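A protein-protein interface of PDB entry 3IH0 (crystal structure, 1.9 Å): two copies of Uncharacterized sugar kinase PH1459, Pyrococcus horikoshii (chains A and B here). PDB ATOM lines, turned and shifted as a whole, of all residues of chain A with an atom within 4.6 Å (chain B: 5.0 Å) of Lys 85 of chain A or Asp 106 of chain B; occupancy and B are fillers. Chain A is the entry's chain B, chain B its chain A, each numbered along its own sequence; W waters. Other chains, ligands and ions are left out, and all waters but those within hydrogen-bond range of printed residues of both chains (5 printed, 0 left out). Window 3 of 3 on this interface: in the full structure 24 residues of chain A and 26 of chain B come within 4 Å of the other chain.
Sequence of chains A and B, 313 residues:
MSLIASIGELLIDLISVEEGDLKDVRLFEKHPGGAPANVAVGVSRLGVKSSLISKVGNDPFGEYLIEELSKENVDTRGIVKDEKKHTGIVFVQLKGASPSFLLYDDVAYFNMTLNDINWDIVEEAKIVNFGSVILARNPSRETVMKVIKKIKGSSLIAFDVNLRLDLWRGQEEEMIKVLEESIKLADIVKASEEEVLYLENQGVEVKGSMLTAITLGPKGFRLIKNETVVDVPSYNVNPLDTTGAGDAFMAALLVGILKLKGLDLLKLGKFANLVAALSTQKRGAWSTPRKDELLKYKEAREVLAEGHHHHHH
The side-chain amino group (NZ) of Lys 85 of chain B lies within salt-bridge range of the side-chain carboxylate (OD1) of Asp 106 of chain A, at 3.5 Å.
The side-chain hydroxyl (OH) of Tyr 104 of chain B sits at hydrogen-bond distance from the backbone carbonyl oxygen (O) of Thr 87 of chain A (2.7 Å).
The side-chain carboxylate of Asp 106 of chain B is in salt-bridge range of the side-chain amino group of Lys 85 of chain A (3.3 Å).
OD2 of Asp 106 of chain A sits close to OD1 of Asp 106 of chain B (2.4 Å).
The side-chain amino group (NZ) of Lys 85 of chain B lies within salt-bridge range of the side-chain carboxylate (OD2) of Asp 106 of chain B (2.8 Å).
The side-chain hydroxyl (OG1) of Thr 87 of chain A is in hydrogen-bond range of the backbone NH (N) of Gly 57 of chain A.
The backbone NH (N) of Lys 85 of chain A lies within hydrogen-bond range of the side-chain carboxylate (OD1) of Asp 82 of chain A (2.8 Å).
NZ of Lys 85 of chain A lies within salt-bridge range of OD2 of Asp 106 of chain A, at 3.7 Å.
N of Ala 108 of chain A sits at hydrogen-bond distance from O of His 86 of chain A.
Of the 6 printed residues of chain B, 4 touch a printed residue of chain A.
Hydrophobic or aromatic side chains of chain A within 4 Å of the printed part of chain B: His 86.
Among the printed residues, Asp or Glu carboxylates within 4 Å of a Lys or Arg side-chain nitrogen of the other chain: Lys 85 of chain A with Asp 106 of chain B and Asp 106 of chain A with Lys 85 of chain B.
Water W4 lies within hydrogen-bond range of OD2 of Asp 106 of chain A (2.5 Å), OD1 of Asp 106 of chain B (2.6 Å), NZ of Lys 85 of chain A (3.1 Å) and NZ of Lys 85 of chain B (3.3 Å).
Water W5 lies within hydrogen-bond range of the side-chain carboxylate of Asp 105 of chain B (2.7 Å) and the backbone carbonyl oxygen of Lys 84 of chain A (2.9 Å).
Water W2 bridges OD2 of Asp 105 of chain B and O of Lys 84 of chain A.
Water W3 bridges the side-chain amino group (NZ) of Lys 85 of chain A (2.9 Å) and the side-chain carboxylate (OD1) of Asp 106 of chain B (3.3 Å).
Water W1 bridges O of Asp 106 of chain A (2.9 Å) and O of Asp 106 of chain B (3.0 Å).
Lys 85 of chain A touches Asp 106 of chain B, and with the chains exchanged Asp 106 of chain A touches Lys 85 of chain B.
Asp 106 of chain B touches its own counterpart, Asp 106 of chain A.
Glu 83 of chain A touches none of the printed residues of chain B.
Lys 85 of chain A touches just one residue of chain B: Asp 106.
Printed residues of chain A within 4 Å of Tyr 104 of chain B: His 86 and Thr 87.
Printed residues of chain A within 4 Å of Asp 105 of chain B: His 86.
Val 107 of chain B touches none of the printed residues of chain A.
The nearest printed residue of chain B that does not touch Lys 85 of chain A is Asp 105 of chain B (5.8 Å).
The nearest printed residue of chain A that does not touch Asp 106 of chain B is His 86 of chain A (5.8 Å).
The nearest printed residue of chain A that does not touch Asp 105 of chain B is Lys 84 of chain A (4.4 Å).
Tyr 104 of chain B touches His 86 of chain A (CE2 to CB, 3.5 Å).
Asp 105 of chain B touches His 86 of chain A.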
ATOM      1  N   GLY A  57      10.851   0.871 -23.000  1.00  0.00           N
ATOM      2  CA  GLY A  57      11.438   0.707 -21.689  1.00  0.00           C
ATOM      3  C   GLY A  57      11.057   1.851 -20.769  1.00  0.00           C
ATOM      4  O   GLY A  57      10.533   2.874 -21.225  1.00  0.00           O
ATOM      5  N   ASN A  58      11.293   1.667 -19.469  1.00  0.00           N
ATOM      6  CA  ASN A  58      11.026   2.710 -18.495  1.00  0.00           C
ATOM      7  C   ASN A  58      12.278   3.585 -18.476  1.00  0.00           C
ATOM      8  O   ASN A  58      13.085   3.539 -17.544  1.00  0.00           O
ATOM      9  CB  ASN A  58      10.770   2.093 -17.118  1.00  0.00           C
ATOM     10  CG  ASN A  58      10.585   3.135 -16.035  1.00  0.00           C
ATOM     11  OD1 ASN A  58      10.126   4.248 -16.300  1.00  0.00           O
ATOM     12  ND2 ASN A  58      10.930   2.772 -14.797  1.00  0.00           N
ATOM     13  N   ASP A  82       8.363  -1.447 -20.151  1.00  0.00           N
ATOM     14  CA  ASP A  82       9.066  -2.610 -19.639  1.00  0.00           C
ATOM     15  C   ASP A  82      10.078  -2.180 -18.571  1.00  0.00           C
ATOM     16  O   ASP A  82      10.905  -1.308 -18.817  1.00  0.00           O
ATOM     17  CB  ASP A  82       9.795  -3.308 -20.785  1.00  0.00           C
ATOM     18  CG  ASP A  82      10.233  -4.716 -20.427  1.00  0.00           C
ATOM     19  OD1 ASP A  82      10.916  -4.892 -19.398  1.00  0.00           O
ATOM     20  OD2 ASP A  82       9.892  -5.648 -21.186  1.00  0.00           O
ATOM     21  N   GLU A  83      10.006  -2.796 -17.393  1.00  0.00           N
ATOM     22  CA  GLU A  83      10.922  -2.455 -16.308  1.00  0.00           C
ATOM     23  C   GLU A  83      12.305  -3.075 -16.453  1.00  0.00           C
ATOM     24  O   GLU A  83      13.272  -2.589 -15.862  1.00  0.00           O
ATOM     25  CB  GLU A  83      10.335  -2.880 -14.965  1.00  0.00           C
ATOM     26  CG  GLU A  83       9.249  -1.965 -14.449  1.00  0.00           C
ATOM     27  CD  GLU A  83       9.700  -0.517 -14.320  1.00  0.00           C
ATOM     28  OE1 GLU A  83      10.921  -0.247 -14.308  1.00  0.00           O
ATOM     29  OE2 GLU A  83       8.815   0.359 -14.222  1.00  0.00           O
ATOM     30  N   LYS A  84      12.402  -4.134 -17.250  1.00  0.00           N
ATOM     31  CA  LYS A  84      13.672  -4.826 -17.432  1.00  0.00           C
ATOM     32  C   LYS A  84      14.406  -4.485 -18.718  1.00  0.00           C
ATOM     33  O   LYS A  84      15.629  -4.337 -18.716  1.00  0.00           O
ATOM     34  CB  LYS A  84      13.443  -6.338 -17.381  1.00  0.00           C
ATOM     35  CG  LYS A  84      12.651  -6.796 -16.160  1.00  0.00           C
ATOM     36  CD  LYS A  84      13.335  -6.391 -14.856  1.00  0.00           C
ATOM     37  CE  LYS A  84      12.568  -6.907 -13.641  1.00  0.00           C
ATOM     38  NZ  LYS A  84      13.251  -6.577 -12.355  1.00  0.00           N
ATOM     39  N   LYS A  85      13.666  -4.351 -19.812  1.00  0.00           N
ATOM     40  CA  LYS A  85      14.270  -4.075 -21.112  1.00  0.00           C
ATOM     41  C   LYS A  85      14.159  -2.607 -21.510  1.00  0.00           C
ATOM     42  O   LYS A  85      13.150  -1.957 -21.258  1.00  0.00           O
ATOM     43  CB  LYS A  85      13.612  -4.949 -22.190  1.00  0.00           C
ATOM     44  CG  LYS A  85      13.553  -6.442 -21.864  1.00  0.00           C
ATOM     45  CD  LYS A  85      14.932  -7.102 -21.897  1.00  0.00           C
ATOM     46  CE  LYS A  85      14.808  -8.616 -21.773  1.00  0.00           C
ATOM     47  NZ  LYS A  85      16.148  -9.278 -21.763  1.00  0.00           N
ATOM     48  N   HIS A  86      15.204  -2.091 -22.135  1.00  0.00           N
ATOM     49  CA  HIS A  86      15.195  -0.708 -22.563  1.00  0.00           C
ATOM     50  C   HIS A  86      14.575  -0.524 -23.948  1.00  0.00           C
ATOM     51  O   HIS A  86      14.440  -1.475 -24.725  1.00  0.00           O
ATOM     52  CB  HIS A  86      16.607  -0.133 -22.543  1.00  0.00           C
ATOM     53  CG  HIS A  86      17.115   0.126 -21.163  1.00  0.00           C
ATOM     54  ND1 HIS A  86      18.029  -0.690 -20.536  1.00  0.00           N
ATOM     55  CD2 HIS A  86      16.775   1.075 -20.254  1.00  0.00           C
ATOM     56  CE1 HIS A  86      18.232  -0.258 -19.303  1.00  0.00           C
ATOM     57  NE2 HIS A  86      17.483   0.811 -19.109  1.00  0.00           N
ATOM     58  N   THR A  87      14.205   0.722 -24.224  1.00  0.00           N
ATOM     59  CA  THR A  87      13.580   1.113 -25.472  1.00  0.00           C
ATOM     60  C   THR A  87      14.376   0.636 -26.672  1.00  0.00           C
ATOM     61  O   THR A  87      15.599   0.713 -26.690  1.00  0.00           O
ATOM     62  CB  THR A  87      13.433   2.636 -25.514  1.00  0.00           C
ATOM     63  OG1 THR A  87      12.692   3.058 -24.361  1.00  0.00           O
ATOM     64  CG2 THR A  87      12.716   3.078 -26.792  1.00  0.00           C
ATOM     65  N   ASP A 106      17.853  -7.044 -28.115  1.00  0.00           N
ATOM     66  CA  ASP A 106      17.492  -7.325 -26.721  1.00  0.00           C
ATOM     67  C   ASP A 106      16.839  -6.073 -26.130  1.00  0.00           C
ATOM     68  O   ASP A 106      17.414  -5.398 -25.273  1.00  0.00           O
ATOM     69  CB  ASP A 106      18.728  -7.719 -25.898  1.00  0.00           C
ATOM     70  CG  ASP A 106      18.855  -9.230 -25.711  1.00  0.00           C
ATOM     71  OD1 ASP A 106      19.524  -9.897 -26.532  1.00  0.00           O
ATOM     72  OD2 ASP A 106      18.270  -9.761 -24.743  1.00  0.00           O
ATOM     73  N   VAL A 107      15.631  -5.773 -26.597  1.00  0.00           N
ATOM     74  CA  VAL A 107      14.914  -4.581 -26.163  1.00  0.00           C
ATOM     75  C   VAL A 107      13.433  -4.812 -25.855  1.00  0.00           C
ATOM     76  O   VAL A 107      12.883  -5.888 -26.096  1.00  0.00           O
ATOM     77  CB  VAL A 107      15.035  -3.460 -27.231  1.00  0.00           C
ATOM     78  CG1 VAL A 107      16.480  -2.997 -27.335  1.00  0.00           C
ATOM     79  CG2 VAL A 107      14.557  -3.982 -28.593  1.00  0.00           C
ATOM     80  N   ALA A 108      12.799  -3.759 -25.353  1.00  0.00           N
ATOM     81  CA  ALA A 108      11.408  -3.783 -24.941  1.00  0.00           C
ATOM     82  C   ALA A 108      10.379  -4.325 -25.921  1.00  0.00           C
ATOM     83  O   ALA A 108       9.627  -5.222 -25.576  1.00  0.00           O
ATOM     84  CB  ALA A 108      10.992  -2.399 -24.496  1.00  0.00           C
ATOM     85  N   ASN A 111       9.960  -7.968 -26.261  1.00  0.00           N
ATOM     86  CA  ASN A 111       9.628  -8.660 -25.020  1.00  0.00           C
ATOM     87  C   ASN A 111       8.145  -8.601 -24.636  1.00  0.00           C
ATOM     88  O   ASN A 111       7.808  -8.601 -23.449  1.00  0.00           O
ATOM     89  CB  ASN A 111      10.495  -8.098 -23.881  1.00  0.00           C
ATOM     90  CG  ASN A 111      10.415  -8.934 -22.617  1.00  0.00           C
ATOM     91  OD1 ASN A 111      10.508 -10.167 -22.665  1.00  0.00           O
ATOM     92  ND2 ASN A 111      10.253  -8.270 -21.476  1.00  0.00           N
ATOM     93  N   LYS B  85      25.066 -11.102 -28.633  1.00  0.00           N
ATOM     94  CA  LYS B  85      24.759  -9.801 -28.032  1.00  0.00           C
ATOM     95  C   LYS B  85      25.472  -8.705 -28.814  1.00  0.00           C
ATOM     96  O   LYS B  85      26.535  -8.938 -29.383  1.00  0.00           O
ATOM     97  CB  LYS B  85      25.216  -9.757 -26.566  1.00  0.00           C
ATOM     98  CG  LYS B  85      24.659 -10.853 -25.679  1.00  0.00           C
ATOM     99  CD  LYS B  85      23.188 -10.664 -25.379  1.00  0.00           C
ATOM    100  CE  LYS B  85      22.730 -11.665 -24.345  1.00  0.00           C
ATOM    101  NZ  LYS B  85      21.307 -11.472 -24.020  1.00  0.00           N
ATOM    102  N   TYR B 104      22.682   0.769 -21.912  1.00  0.00           N
ATOM    103  CA  TYR B 104      21.952  -0.408 -22.344  1.00  0.00           C
ATOM    104  C   TYR B 104      22.675  -1.554 -21.685  1.00  0.00           C
ATOM    105  O   TYR B 104      23.862  -1.756 -21.919  1.00  0.00           O
ATOM    106  CB  TYR B 104      21.965  -0.509 -23.864  1.00  0.00           C
ATOM    107  CG  TYR B 104      20.818   0.265 -24.445  1.00  0.00           C
ATOM    108  CD1 TYR B 104      20.751   1.650 -24.293  1.00  0.00           C
ATOM    109  CD2 TYR B 104      19.730  -0.390 -25.019  1.00  0.00           C
ATOM    110  CE1 TYR B 104      19.633   2.357 -24.684  1.00  0.00           C
ATOM    111  CE2 TYR B 104      18.603   0.316 -25.412  1.00  0.00           C
ATOM    112  CZ  TYR B 104      18.561   1.690 -25.237  1.00  0.00           C
ATOM    113  OH  TYR B 104      17.437   2.408 -25.592  1.00  0.00           O
ATOM    114  N   ASP B 105      21.973  -2.292 -20.836  1.00  0.00           N
ATOM    115  CA  ASP B 105      22.641  -3.359 -20.116  1.00  0.00           C
ATOM    116  C   ASP B 105      22.676  -4.729 -20.776  1.00  0.00           C
ATOM    117  O   ASP B 105      23.528  -5.553 -20.433  1.00  0.00           O
ATOM    118  CB  ASP B 105      22.069  -3.444 -18.698  1.00  0.00           C
ATOM    119  CG  ASP B 105      20.617  -3.889 -18.671  1.00  0.00           C
ATOM    120  OD1 ASP B 105      19.866  -3.572 -19.617  1.00  0.00           O
ATOM    121  OD2 ASP B 105      20.230  -4.551 -17.690  1.00  0.00           O
ATOM    122  N   ASP B 106      21.788  -4.995 -21.727  1.00  0.00           N
ATOM    123  CA  ASP B 106      21.837  -6.305 -22.342  1.00  0.00           C
ATOM    124  C   ASP B 106      22.704  -6.229 -23.585  1.00  0.00           C
ATOM    125  O   ASP B 106      22.222  -6.220 -24.724  1.00  0.00           O
ATOM    126  CB  ASP B 106      20.434  -6.821 -22.662  1.00  0.00           C
ATOM    127  CG  ASP B 106      20.389  -8.338 -22.721  1.00  0.00           C
ATOM    128  OD1 ASP B 106      19.276  -8.901 -22.710  1.00  0.00           O
ATOM    129  OD2 ASP B 106      21.475  -8.965 -22.780  1.00  0.00           O
ATOM    130  N   VAL B 107      24.005  -6.168 -23.329  1.00  0.00           N
ATOM    131  CA  VAL B 107      25.001  -6.053 -24.370  1.00  0.00           C
ATOM    132  C   VAL B 107      26.173  -7.016 -24.151  1.00  0.00           C
ATOM    133  O   VAL B 107      26.306  -7.624 -23.087  1.00  0.00           O
ATOM    134  CB  VAL B 107      25.491  -4.615 -24.423  1.00  0.00           C
ATOM    135  CG1 VAL B 107      24.349  -3.712 -24.863  1.00  0.00           C
ATOM    136  CG2 VAL B 107      25.970  -4.199 -23.038  1.00  0.00           C
ATOM    137  N   ALA B 108      27.026  -7.128 -25.161  1.00  0.00           N
ATOM    138  CA  ALA B 108      28.139  -8.062 -25.133  1.00  0.00           C
ATOM    139  C   ALA B 108      29.082  -8.050 -23.928  1.00  0.00           C
ATOM    140  O   ALA B 108      29.382  -9.107 -23.387  1.00  0.00           O
ATOM    141  CB  ALA B 108      28.952  -7.939 -26.433  1.00  0.00           C
HETATM  142  O   HOH W   1      20.128  -4.326 -25.705  1.00  0.00           O
HETATM  143  O   HOH W   2      17.694  -3.971 -16.914  1.00  0.00           O
HETATM  144  O   HOH W   3      17.961  -8.098 -19.805  1.00  0.00           O
HETATM  145  O   HOH W   4      18.233 -11.262 -22.798  1.00  0.00           O
HETATM  146  O   HOH W   5      17.834  -5.127 -20.347  1.00  0.00           O
